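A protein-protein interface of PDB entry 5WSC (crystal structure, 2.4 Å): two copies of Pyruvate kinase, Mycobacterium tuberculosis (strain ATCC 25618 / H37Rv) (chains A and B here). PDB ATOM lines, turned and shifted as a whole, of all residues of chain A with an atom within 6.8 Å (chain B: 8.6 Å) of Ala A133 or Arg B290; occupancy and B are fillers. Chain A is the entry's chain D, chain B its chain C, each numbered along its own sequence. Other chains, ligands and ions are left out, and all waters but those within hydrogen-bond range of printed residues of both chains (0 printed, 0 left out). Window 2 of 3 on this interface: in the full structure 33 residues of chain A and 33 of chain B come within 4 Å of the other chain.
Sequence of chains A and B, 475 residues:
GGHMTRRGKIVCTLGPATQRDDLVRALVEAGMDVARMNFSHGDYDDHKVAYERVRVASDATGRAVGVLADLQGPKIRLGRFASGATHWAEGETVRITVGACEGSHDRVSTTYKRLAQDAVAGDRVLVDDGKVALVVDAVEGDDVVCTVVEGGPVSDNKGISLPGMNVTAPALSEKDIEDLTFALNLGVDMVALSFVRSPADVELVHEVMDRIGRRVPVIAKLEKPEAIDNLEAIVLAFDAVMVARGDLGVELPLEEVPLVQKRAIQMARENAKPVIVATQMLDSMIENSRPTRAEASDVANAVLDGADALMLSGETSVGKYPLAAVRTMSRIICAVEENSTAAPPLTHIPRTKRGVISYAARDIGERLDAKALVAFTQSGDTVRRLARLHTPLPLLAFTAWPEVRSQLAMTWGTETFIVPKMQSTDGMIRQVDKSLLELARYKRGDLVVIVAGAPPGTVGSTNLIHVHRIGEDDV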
ATOM      1  N   ARG A 124      -0.628  22.821 -18.337  1.00  0.00           N
ATOM      2  CA  ARG A 124       0.824  22.834 -18.380  1.00  0.00           C
ATOM      3  C   ARG A 124       1.281  23.868 -19.395  1.00  0.00           C
ATOM      4  O   ARG A 124       0.543  24.243 -20.307  1.00  0.00           O
ATOM      5  CB  ARG A 124       1.384  21.428 -18.666  1.00  0.00           C
ATOM      6  CG  ARG A 124       1.132  20.451 -17.492  1.00  0.00           C
ATOM      7  CD  ARG A 124       1.628  19.029 -17.752  1.00  0.00           C
ATOM      8  NE  ARG A 124       0.939  18.362 -18.853  1.00  0.00           N
ATOM      9  CZ  ARG A 124      -0.185  17.649 -18.732  1.00  0.00           C
ATOM     10  NH1 ARG A 124      -0.781  17.513 -17.554  1.00  0.00           N
ATOM     11  NH2 ARG A 124      -0.732  17.096 -19.804  1.00  0.00           N
ATOM     12  N   VAL A 125       2.466  24.414 -19.157  1.00  0.00           N
ATOM     13  CA  VAL A 125       3.027  25.439 -20.026  1.00  0.00           C
ATOM     14  C   VAL A 125       4.446  25.010 -20.246  1.00  0.00           C
ATOM     15  O   VAL A 125       5.246  25.047 -19.311  1.00  0.00           O
ATOM     16  CB  VAL A 125       3.036  26.846 -19.349  1.00  0.00           C
ATOM     17  CG1 VAL A 125       3.668  27.867 -20.259  1.00  0.00           C
ATOM     18  CG2 VAL A 125       1.623  27.275 -18.944  1.00  0.00           C
ATOM     19  N   LEU A 126       4.759  24.561 -21.464  1.00  0.00           N
ATOM     20  CA  LEU A 126       6.134  24.207 -21.820  1.00  0.00           C
ATOM     21  C   LEU A 126       6.733  25.374 -22.564  1.00  0.00           C
ATOM     22  O   LEU A 126       6.127  25.883 -23.479  1.00  0.00           O
ATOM     23  CB  LEU A 126       6.182  22.989 -22.729  1.00  0.00           C
ATOM     24  CG  LEU A 126       5.700  21.652 -22.234  1.00  0.00           C
ATOM     25  CD1 LEU A 126       5.988  21.464 -20.756  1.00  0.00           C
ATOM     26  CD2 LEU A 126       4.227  21.546 -22.518  1.00  0.00           C
ATOM     27  N   VAL A 127       7.937  25.786 -22.174  1.00  0.00           N
ATOM     28  CA  VAL A 127       8.556  26.977 -22.718  1.00  0.00           C
ATOM     29  C   VAL A 127       9.752  26.547 -23.525  1.00  0.00           C
ATOM     30  O   VAL A 127      10.528  25.678 -23.121  1.00  0.00           O
ATOM     31  CB  VAL A 127       9.068  27.928 -21.594  1.00  0.00           C
ATOM     32  CG1 VAL A 127       9.640  29.198 -22.186  1.00  0.00           C
ATOM     33  CG2 VAL A 127       7.966  28.240 -20.606  1.00  0.00           C
ATOM     34  N   ASP A 129      10.222  24.891 -26.269  1.00  0.00           N
ATOM     35  CA  ASP A 129      10.140  23.472 -26.570  1.00  0.00           C
ATOM     36  C   ASP A 129      10.526  22.529 -25.399  1.00  0.00           C
ATOM     37  O   ASP A 129      10.864  21.354 -25.601  1.00  0.00           O
ATOM     38  CB  ASP A 129      10.880  23.187 -27.879  1.00  0.00           C
ATOM     39  CG  ASP A 129      10.151  23.793 -29.101  1.00  0.00           C
ATOM     40  OD1 ASP A 129       8.937  24.075 -29.004  1.00  0.00           O
ATOM     41  OD2 ASP A 129      10.763  24.017 -30.141  1.00  0.00           O
ATOM     42  N   GLY A 130      10.372  23.035 -24.173  1.00  0.00           N
ATOM     43  CA  GLY A 130      10.356  22.173 -22.987  1.00  0.00           C
ATOM     44  C   GLY A 130      11.578  22.297 -22.106  1.00  0.00           C
ATOM     45  O   GLY A 130      11.751  21.477 -21.195  1.00  0.00           O
ATOM     46  N   LYS A 131      12.426  23.313 -22.345  1.00  0.00           N
ATOM     47  CA  LYS A 131      13.567  23.517 -21.429  1.00  0.00           C
ATOM     48  C   LYS A 131      13.120  24.098 -20.121  1.00  0.00           C
ATOM     49  O   LYS A 131      13.889  24.129 -19.172  1.00  0.00           O
ATOM     50  CB  LYS A 131      14.759  24.232 -22.065  1.00  0.00           C
ATOM     51  CG  LYS A 131      15.675  23.234 -22.820  1.00  0.00           C
ATOM     52  CD  LYS A 131      14.845  22.154 -23.537  1.00  0.00           C
ATOM     53  CE  LYS A 131      15.661  21.043 -24.165  1.00  0.00           C
ATOM     54  NZ  LYS A 131      14.709  20.019 -24.703  1.00  0.00           N
ATOM     55  N   VAL A 132      11.865  24.532 -20.067  1.00  0.00           N
ATOM     56  CA  VAL A 132      11.214  24.885 -18.802  1.00  0.00           C
ATOM     57  C   VAL A 132       9.753  24.447 -18.856  1.00  0.00           C
ATOM     58  O   VAL A 132       9.083  24.634 -19.876  1.00  0.00           O
ATOM     59  CB  VAL A 132      11.245  26.415 -18.582  1.00  0.00           C
ATOM     60  CG1 VAL A 132      10.268  26.850 -17.471  1.00  0.00           C
ATOM     61  CG2 VAL A 132      12.644  26.861 -18.281  1.00  0.00           C
ATOM     62  N   ALA A 133       9.233  23.904 -17.766  1.00  0.00           N
ATOM     63  CA  ALA A 133       7.794  23.573 -17.704  1.00  0.00           C
ATOM     64  C   ALA A 133       7.163  24.185 -16.459  1.00  0.00           C
ATOM     65  O   ALA A 133       7.772  24.166 -15.371  1.00  0.00           O
ATOM     66  CB  ALA A 133       7.584  22.065 -17.716  1.00  0.00           C
ATOM     67  N   LEU A 134       5.960  24.727 -16.637  1.00  0.00           N
ATOM     68  CA  LEU A 134       5.192  25.331 -15.554  1.00  0.00           C
ATOM     69  C   LEU A 134       3.792  24.704 -15.476  1.00  0.00           C
ATOM     70  O   LEU A 134       3.311  24.130 -16.437  1.00  0.00           O
ATOM     71  CB  LEU A 134       5.044  26.845 -15.750  1.00  0.00           C
ATOM     72  CG  LEU A 134       6.133  27.615 -16.521  1.00  0.00           C
ATOM     73  CD1 LEU A 134       5.564  28.890 -17.087  1.00  0.00           C
ATOM     74  CD2 LEU A 134       7.349  27.922 -15.677  1.00  0.00           C
ATOM     75  N   VAL A 135       3.150  24.821 -14.323  1.00  0.00           N
ATOM     76  CA  VAL A 135       1.780  24.363 -14.172  1.00  0.00           C
ATOM     77  C   VAL A 135       0.942  25.530 -13.684  1.00  0.00           C
ATOM     78  O   VAL A 135       1.371  26.296 -12.851  1.00  0.00           O
ATOM     79  CB  VAL A 135       1.686  23.142 -13.222  1.00  0.00           C
ATOM     80  CG1 VAL A 135       0.248  22.764 -12.933  1.00  0.00           C
ATOM     81  CG2 VAL A 135       2.409  21.947 -13.826  1.00  0.00           C
ATOM     82  N   THR A 147       3.439  27.666 -11.290  1.00  0.00           N
ATOM     83  CA  THR A 147       4.589  27.189 -10.573  1.00  0.00           C
ATOM     84  C   THR A 147       5.532  26.548 -11.552  1.00  0.00           C
ATOM     85  O   THR A 147       5.097  25.752 -12.393  1.00  0.00           O
ATOM     86  CB  THR A 147       4.170  26.160  -9.511  1.00  0.00           C
ATOM     87  OG1 THR A 147       3.200  26.749  -8.641  1.00  0.00           O
ATOM     88  CG2 THR A 147       5.315  25.734  -8.696  1.00  0.00           C
ATOM     89  N   VAL A 148       6.823  26.883 -11.430  1.00  0.00           N
ATOM     90  CA  VAL A 148       7.849  26.229 -12.252  1.00  0.00           C
ATOM     91  C   VAL A 148       8.037  24.838 -11.710  1.00  0.00           C
ATOM     92  O   VAL A 148       8.337  24.679 -10.526  1.00  0.00           O
ATOM     93  CB  VAL A 148       9.201  26.991 -12.244  1.00  0.00           C
ATOM     94  CG1 VAL A 148      10.185  26.325 -13.172  1.00  0.00           C
ATOM     95  CG2 VAL A 148       9.024  28.444 -12.707  1.00  0.00           C
ATOM     96  N   VAL A 149       7.808  23.839 -12.568  1.00  0.00           N
ATOM     97  CA  VAL A 149       7.878  22.435 -12.218  1.00  0.00           C
ATOM     98  C   VAL A 149       9.126  21.786 -12.824  1.00  0.00           C
ATOM     99  O   VAL A 149       9.618  20.776 -12.344  1.00  0.00           O
ATOM    100  CB  VAL A 149       6.618  21.698 -12.729  1.00  0.00           C
ATOM    101  CG1 VAL A 149       6.843  20.198 -12.780  1.00  0.00           C
ATOM    102  CG2 VAL A 149       5.421  22.016 -11.848  1.00  0.00           C
ATOM    103  N   GLU A 150       9.649  22.369 -13.897  1.00  0.00           N
ATOM    104  CA  GLU A 150      10.982  22.010 -14.354  1.00  0.00           C
ATOM    105  C   GLU A 150      11.702  23.255 -14.735  1.00  0.00           C
ATOM    106  O   GLU A 150      11.254  23.964 -15.607  1.00  0.00           O
ATOM    107  CB  GLU A 150      10.896  21.100 -15.574  1.00  0.00           C
ATOM    108  CG  GLU A 150       9.824  20.044 -15.501  1.00  0.00           C
ATOM    109  CD  GLU A 150       9.890  19.201 -16.730  1.00  0.00           C
ATOM    110  OE1 GLU A 150       9.646  17.974 -16.635  1.00  0.00           O
ATOM    111  OE2 GLU A 150      10.242  19.793 -17.773  1.00  0.00           O
ATOM    112  N   GLY A 151      12.849  23.489 -14.119  1.00  0.00           N
ATOM    113  CA  GLY A 151      13.522  24.774 -14.259  1.00  0.00           C
ATOM    114  C   GLY A 151      14.527  24.849 -15.384  1.00  0.00           C
ATOM    115  O   GLY A 151      15.071  23.855 -15.806  1.00  0.00           O
ATOM    116  N   GLY A 152      14.805  26.062 -15.832  1.00  0.00           N
ATOM    117  CA  GLY A 152      15.687  26.287 -16.976  1.00  0.00           C
ATOM    118  C   GLY A 152      15.775  27.783 -17.264  1.00  0.00           C
ATOM    119  O   GLY A 152      14.980  28.565 -16.739  1.00  0.00           O
ATOM    120  N   GLY A 249       7.239  17.919 -30.378  1.00  0.00           N
ATOM    121  CA  GLY A 249       7.573  17.245 -29.143  1.00  0.00           C
ATOM    122  C   GLY A 249       7.044  17.865 -27.869  1.00  0.00           C
ATOM    123  O   GLY A 249       7.216  17.293 -26.823  1.00  0.00           O
ATOM    124  N   VAL A 250       6.411  19.033 -27.934  1.00  0.00           N
ATOM    125  CA  VAL A 250       5.651  19.525 -26.779  1.00  0.00           C
ATOM    126  C   VAL A 250       4.149  19.589 -27.039  1.00  0.00           C
ATOM    127  O   VAL A 250       3.339  19.612 -26.104  1.00  0.00           O
ATOM    128  CB  VAL A 250       6.150  20.903 -26.319  1.00  0.00           C
ATOM    129  CG1 VAL A 250       7.521  20.777 -25.686  1.00  0.00           C
ATOM    130  CG2 VAL A 250       6.189  21.892 -27.467  1.00  0.00           C
ATOM    131  N   LEU A 254       6.649  13.676 -26.243  1.00  0.00           N
ATOM    132  CA  LEU A 254       7.878  13.619 -26.986  1.00  0.00           C
ATOM    133  C   LEU A 254       8.223  12.192 -27.342  1.00  0.00           C
ATOM    134  O   LEU A 254       8.974  11.957 -28.274  1.00  0.00           O
ATOM    135  CB  LEU A 254       9.024  14.311 -26.229  1.00  0.00           C
ATOM    136  CG  LEU A 254       9.523  13.789 -24.891  1.00  0.00           C
ATOM    137  CD1 LEU A 254      10.262  12.467 -25.030  1.00  0.00           C
ATOM    138  CD2 LEU A 254      10.501  14.826 -24.305  1.00  0.00           C
ATOM    139  N   LEU B 282      20.588   9.542 -23.516  1.00  0.00           N
ATOM    140  CA  LEU B 282      19.827  10.662 -23.001  1.00  0.00           C
ATOM    141  C   LEU B 282      20.754  11.695 -22.412  1.00  0.00           C
ATOM    142  O   LEU B 282      20.405  12.409 -21.474  1.00  0.00           O
ATOM    143  CB  LEU B 282      18.775  10.190 -21.995  1.00  0.00           C
ATOM    144  CG  LEU B 282      17.698   9.323 -22.606  1.00  0.00           C
ATOM    145  CD1 LEU B 282      16.751   8.812 -21.549  1.00  0.00           C
ATOM    146  CD2 LEU B 282      16.945  10.053 -23.696  1.00  0.00           C
ATOM    147  N   ASP B 283      21.910  11.842 -23.018  1.00  0.00           N
ATOM    148  CA  ASP B 283      22.959  12.689 -22.446  1.00  0.00           C
ATOM    149  C   ASP B 283      22.519  14.009 -21.824  1.00  0.00           C
ATOM    150  O   ASP B 283      23.031  14.364 -20.777  1.00  0.00           O
ATOM    151  CB  ASP B 283      24.025  13.030 -23.483  1.00  0.00           C
ATOM    152  CG  ASP B 283      25.230  13.647 -22.844  1.00  0.00           C
ATOM    153  OD1 ASP B 283      26.030  12.882 -22.254  1.00  0.00           O
ATOM    154  OD2 ASP B 283      25.330  14.894 -22.837  1.00  0.00           O
ATOM    155  N   SER B 284      21.658  14.776 -22.508  1.00  0.00           N
ATOM    156  CA  SER B 284      21.290  16.120 -22.045  1.00  0.00           C
ATOM    157  C   SER B 284      20.496  16.092 -20.736  1.00  0.00           C
ATOM    158  O   SER B 284      20.393  17.096 -20.048  1.00  0.00           O
ATOM    159  CB  SER B 284      20.504  16.870 -23.125  1.00  0.00           C
ATOM    160  OG  SER B 284      19.131  16.494 -23.177  1.00  0.00           O
ATOM    161  N   MET B 285      19.920  14.956 -20.384  1.00  0.00           N
ATOM    162  CA  MET B 285      19.166  14.889 -19.155  1.00  0.00           C
ATOM    163  C   MET B 285      20.070  14.876 -17.927  1.00  0.00           C
ATOM    164  O   MET B 285      19.585  14.877 -16.779  1.00  0.00           O
ATOM    165  CB  MET B 285      18.280  13.660 -19.125  1.00  0.00           C
ATOM    166  CG  MET B 285      17.286  13.621 -20.229  1.00  0.00           C
ATOM    167  SD  MET B 285      15.979  12.496 -19.767  1.00  0.00           S
ATOM    168  CE  MET B 285      15.224  13.417 -18.386  1.00  0.00           C
ATOM    169  N   ILE B 286      21.373  14.851 -18.142  1.00  0.00           N
ATOM    170  CA  ILE B 286      22.304  15.121 -17.060  1.00  0.00           C
ATOM    171  C   ILE B 286      21.976  16.470 -16.423  1.00  0.00           C
ATOM    172  O   ILE B 286      22.021  16.597 -15.204  1.00  0.00           O
ATOM    173  CB  ILE B 286      23.782  15.082 -17.555  1.00  0.00           C
ATOM    174  CG1 ILE B 286      24.153  13.622 -17.842  1.00  0.00           C
ATOM    175  CG2 ILE B 286      24.747  15.656 -16.512  1.00  0.00           C
ATOM    176  CD1 ILE B 286      25.553  13.368 -18.358  1.00  0.00           C
ATOM    177  N   GLU B 287      21.620  17.454 -17.258  1.00  0.00           N
ATOM    178  CA  GLU B 287      21.376  18.824 -16.817  1.00  0.00           C
ATOM    179  C   GLU B 287      19.939  19.279 -17.035  1.00  0.00           C
ATOM    180  O   GLU B 287      19.545  20.331 -16.530  1.00  0.00           O
ATOM    181  CB  GLU B 287      22.294  19.788 -17.568  1.00  0.00           C
ATOM    182  CG  GLU B 287      23.781  19.595 -17.267  1.00  0.00           C
ATOM    183  CD  GLU B 287      24.098  19.904 -15.844  1.00  0.00           C
ATOM    184  OE1 GLU B 287      25.250  19.735 -15.366  1.00  0.00           O
ATOM    185  OE2 GLU B 287      23.150  20.302 -15.187  1.00  0.00           O
ATOM    186  N   ASN B 288      19.154  18.519 -17.797  1.00  0.00           N
ATOM    187  CA  ASN B 288      17.794  18.953 -18.151  1.00  0.00           C
ATOM    188  C   ASN B 288      16.768  17.889 -17.808  1.00  0.00           C
ATOM    189  O   ASN B 288      17.063  16.678 -17.814  1.00  0.00           O
ATOM    190  CB  ASN B 288      17.703  19.215 -19.654  1.00  0.00           C
ATOM    191  CG  ASN B 288      18.622  20.338 -20.133  1.00  0.00           C
ATOM    192  OD1 ASN B 288      18.139  21.430 -20.447  1.00  0.00           O
ATOM    193  ND2 ASN B 288      19.937  20.029 -20.311  1.00  0.00           N
ATOM    194  N   SER B 289      15.542  18.336 -17.562  1.00  0.00           N
ATOM    195  CA  SER B 289      14.467  17.452 -17.116  1.00  0.00           C
ATOM    196  C   SER B 289      13.816  16.685 -18.284  1.00  0.00           C
ATOM    197  O   SER B 289      13.064  15.716 -18.075  1.00  0.00           O
ATOM    198  CB  SER B 289      13.424  18.270 -16.343  1.00  0.00           C
ATOM    199  OG  SER B 289      13.063  19.441 -17.045  1.00  0.00           O
ATOM    200  N   ARG B 290      14.122  17.125 -19.510  1.00  0.00           N
ATOM    201  CA  ARG B 290      13.607  16.522 -20.726  1.00  0.00           C
ATOM    202  C   ARG B 290      14.745  16.468 -21.739  1.00  0.00           C
ATOM    203  O   ARG B 290      15.600  17.336 -21.745  1.00  0.00           O
ATOM    204  CB  ARG B 290      12.455  17.349 -21.300  1.00  0.00           C
ATOM    205  CG  ARG B 290      11.177  17.140 -20.560  1.00  0.00           C
ATOM    206  CD  ARG B 290      10.077  18.080 -21.052  1.00  0.00           C
ATOM    207  NE  ARG B 290       9.152  18.387 -19.946  1.00  0.00           N
ATOM    208  CZ  ARG B 290       7.846  18.141 -19.933  1.00  0.00           C
ATOM    209  NH1 ARG B 290       7.224  17.628 -21.013  1.00  0.00           N
ATOM    210  NH2 ARG B 290       7.150  18.451 -18.827  1.00  0.00           N
ATOM    211  N   PRO B 291      14.746  15.437 -22.603  1.00  0.00           N
ATOM    212  CA  PRO B 291      15.806  15.239 -23.572  1.00  0.00           C
ATOM    213  C   PRO B 291      15.535  15.958 -24.901  1.00  0.00           C
ATOM    214  O   PRO B 291      14.435  16.494 -25.129  1.00  0.00           O
ATOM    215  CB  PRO B 291      15.776  13.734 -23.781  1.00  0.00           C
ATOM    216  CG  PRO B 291      14.334  13.391 -23.657  1.00  0.00           C
ATOM    217  CD  PRO B 291      13.833  14.279 -22.562  1.00  0.00           C
ATOM    218  N   THR B 292      16.557  15.980 -25.748  1.00  0.00           N
ATOM    219  CA  THR B 292      16.427  16.500 -27.089  1.00  0.00           C
ATOM    220  C   THR B 292      15.614  15.516 -27.940  1.00  0.00           C
ATOM    221  O   THR B 292      15.303  14.367 -27.518  1.00  0.00           O
ATOM    222  CB  THR B 292      17.803  16.729 -27.739  1.00  0.00           C
ATOM    223  OG1 THR B 292      18.406  15.480 -28.045  1.00  0.00           O
ATOM    224  CG2 THR B 292      18.724  17.468 -26.798  1.00  0.00           C
ATOM    225  N   ARG B 293      15.256  15.974 -29.130  1.00  0.00           N
ATOM    226  CA  ARG B 293      14.517  15.162 -30.091  1.00  0.00           C
ATOM    227  C   ARG B 293      15.401  14.054 -30.658  1.00  0.00           C
ATOM    228  O   ARG B 293      14.905  12.972 -30.948  1.00  0.00           O
ATOM    229  CB  ARG B 293      14.051  16.047 -31.212  1.00  0.00           C
ATOM    230  CG  ARG B 293      13.119  17.145 -30.765  1.00  0.00           C
ATOM    231  CD  ARG B 293      11.906  16.568 -30.059  1.00  0.00           C
ATOM    232  NE  ARG B 293      11.124  17.656 -29.515  1.00  0.00           N
ATOM    233  CZ  ARG B 293      11.194  18.089 -28.265  1.00  0.00           C
ATOM    234  NH1 ARG B 293      11.950  17.454 -27.353  1.00  0.00           N
ATOM    235  NH2 ARG B 293      10.447  19.136 -27.917  1.00  0.00           N
ATOM    236  N   GLU B 295      17.854  12.586 -28.930  1.00  0.00           N
ATOM    237  CA  GLU B 295      17.939  11.592 -27.863  1.00  0.00           C
ATOM    238  C   GLU B 295      16.738  10.667 -27.893  1.00  0.00           C
ATOM    239  O   GLU B 295      16.890   9.450 -27.958  1.00  0.00           O
ATOM    240  CB  GLU B 295      18.134  12.273 -26.535  1.00  0.00           C
ATOM    241  CG  GLU B 295      19.560  12.750 -26.364  1.00  0.00           C
ATOM    242  CD  GLU B 295      19.745  13.853 -25.329  1.00  0.00           C
ATOM    243  OE1 GLU B 295      18.751  14.275 -24.661  1.00  0.00           O
ATOM    244  OE2 GLU B 295      20.918  14.265 -25.179  1.00  0.00           O
ATOM    245  N   ALA B 296      15.545  11.234 -27.906  1.00  0.00           N
ATOM    246  CA  ALA B 296      14.305  10.434 -27.941  1.00  0.00           C
ATOM    247  C   ALA B 296      14.341   9.489 -29.142  1.00  0.00           C
ATOM    248  O   ALA B 296      14.089   8.287 -29.030  1.00  0.00           O
ATOM    249  CB  ALA B 296      13.115  11.345 -28.031  1.00  0.00           C
ATOM    250  N   TYR B 321      19.026  14.487 -12.858  1.00  0.00           N
ATOM    251  CA  TYR B 321      17.690  13.903 -12.975  1.00  0.00           C
ATOM    252  C   TYR B 321      17.687  12.413 -13.212  1.00  0.00           C
ATOM    253  O   TYR B 321      17.143  11.961 -14.209  1.00  0.00           O
ATOM    254  CB  TYR B 321      16.900  14.581 -14.087  1.00  0.00           C
ATOM    255  CG  TYR B 321      16.711  16.081 -13.899  1.00  0.00           C
ATOM    256  CD1 TYR B 321      15.772  16.584 -13.013  1.00  0.00           C
ATOM    257  CD2 TYR B 321      17.502  16.993 -14.609  1.00  0.00           C
ATOM    258  CE1 TYR B 321      15.621  17.949 -12.842  1.00  0.00           C
ATOM    259  CE2 TYR B 321      17.337  18.344 -14.473  1.00  0.00           C
ATOM    260  CZ  TYR B 321      16.394  18.819 -13.579  1.00  0.00           C
ATOM    261  OH  TYR B 321      16.224  20.163 -13.409  1.00  0.00           O
ATOM    262  N   ALA B 324      14.172  10.764 -13.467  1.00  0.00           N
ATOM    263  CA  ALA B 324      13.452  11.201 -14.666  1.00  0.00           C
ATOM    264  C   ALA B 324      14.083  10.565 -15.894  1.00  0.00           C
ATOM    265  O   ALA B 324      13.390  10.210 -16.854  1.00  0.00           O
ATOM    266  CB  ALA B 324      13.440  12.718 -14.780  1.00  0.00           C
ATOM    267  N   ALA B 325      15.405  10.416 -15.868  1.00  0.00           N
ATOM    268  CA  ALA B 325      16.105   9.747 -16.953  1.00  0.00           C
ATOM    269  C   ALA B 325      15.571   8.345 -17.179  1.00  0.00           C
ATOM    270  O   ALA B 325      15.387   7.910 -18.314  1.00  0.00           O
ATOM    271  CB  ALA B 325      17.598   9.694 -16.683  1.00  0.00           C
ATOM    272  N   THR B 328      11.833   8.330 -18.356  1.00  0.00           N
ATOM    273  CA  THR B 328      11.713   8.861 -19.713  1.00  0.00           C
ATOM    274  C   THR B 328      12.089   7.789 -20.704  1.00  0.00           C
ATOM    275  O   THR B 328      11.336   7.493 -21.622  1.00  0.00           O
ATOM    276  CB  THR B 328      12.582  10.112 -19.920  1.00  0.00           C
ATOM    277  OG1 THR B 328      12.181  11.135 -19.013  1.00  0.00           O
ATOM    278  CG2 THR B 328      12.443  10.617 -21.307  1.00  0.00           C
ATOM    279  N   ARG B 331       9.317   5.394 -20.929  1.00  0.00           N
ATOM    280  CA  ARG B 331       8.188   5.857 -21.715  1.00  0.00           C
ATOM    281  C   ARG B 331       8.391   5.751 -23.215  1.00  0.00           C
ATOM    282  O   ARG B 331       7.471   5.373 -23.949  1.00  0.00           O
ATOM    283  CB  ARG B 331       7.774   7.272 -21.306  1.00  0.00           C
ATOM    284  CG  ARG B 331       6.970   7.312 -20.006  1.00  0.00           C
ATOM    285  CD  ARG B 331       6.316   8.687 -19.785  1.00  0.00           C
ATOM    286  NE  ARG B 331       7.317   9.743 -19.635  1.00  0.00           N
ATOM    287  CZ  ARG B 331       7.936  10.032 -18.483  1.00  0.00           C
ATOM    288  NH1 ARG B 331       7.647   9.349 -17.363  1.00  0.00           N
ATOM    289  NH2 ARG B 331       8.849  11.017 -18.427  1.00  0.00           N
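The side-chain hydroxyl of Ser B289 sits at hydrogen-bond distance from the side-chain carboxylate of Glu A150 (2.9 Å). The side-chain carboxylate (OE2) of Glu A150 is in salt-bridge range of the guanidinium group (NE) of Arg B290, 2.8 Å away. NH2 of Arg B293 sits at hydrogen-bond distance from O of Asp A129, 3.2 Å away.
The backbone carbonyl oxygen (O) of Ser B284 lies within hydrogen-bond range of the side-chain amide nitrogen (ND2) of Asn B288, at 3.0 Å. The backbone carbonyl oxygen of Pro B291 is in hydrogen-bond range of the guanidinium group of Arg B293, 3.5 Å away. The backbone carbonyl oxygen (O) of Ala A133 is in hydrogen-bond range of the backbone NH (N) of Val A149, 2.8 Å away. The backbone NH (N) of Ala A133 sits at hydrogen-bond distance from the backbone carbonyl oxygen (O) of Glu A150 (3.0 Å).
Leu A126 touches Arg B290. O of Gly A130 touches CD of Arg B290, 3.8 Å away. Asn B288 touches Lys A131. Pro B291 touches Lys A131 (O to NZ, 3.6 Å). CB of Ala A133 touches NH2 of Arg B290 (3.8 Å). Arg B293 touches Gly A249. Pro B291 touches Leu A254.
Of the printed residues of chain B, Leu A126 touches Arg B290. Printed residues of chain B within 4 Å of Gly A130: Arg B290 (3.8 Å). Printed residues of chain B within 4 Å of Lys A131: Asn B288 and Pro B291. Ala A133 touches one residue of chain B. Of the printed residues of chain B, Glu A150 touches Ser B289 (2.9 Å) and Arg B290 (2.8 Å). Gly A151 touches none of the printed residues of chain B. Printed residues of chain A within 4 Å of Ser B289: Glu A150. Of the printed residues of chain A, Arg B290 touches Leu A126, Gly A130, Ala A133 and Glu A150. Of the printed residues of chain A, Pro B291 touches Lys A131 (3.6 Å) and Leu A254 (3.8 Å). The nearest residue of chain B that does not touch Ala A133 is Ser B289 (5.9 Å).
Hydrophobic or aromatic side chains of chain A that line the printed part of chain B: Leu A126, Ala A133 and Leu A254. Of the 19 printed residues of chain B, 5 touch a printed residue of chain A. Printed residues of chain B that touch a printed residue of chain A: Asn B288, Ser B289, Arg B290, Pro B291 and Arg B293. Hydrophobic or aromatic side chains of chain B that line the printed part of chain A: Pro B291. Among the printed residues, Asp or Glu carboxylates within 4 Å of a Lys or Arg side-chain nitrogen of the other chain: Glu A150 with Arg B290 (2.8 Å).
No position is printed for both chains.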
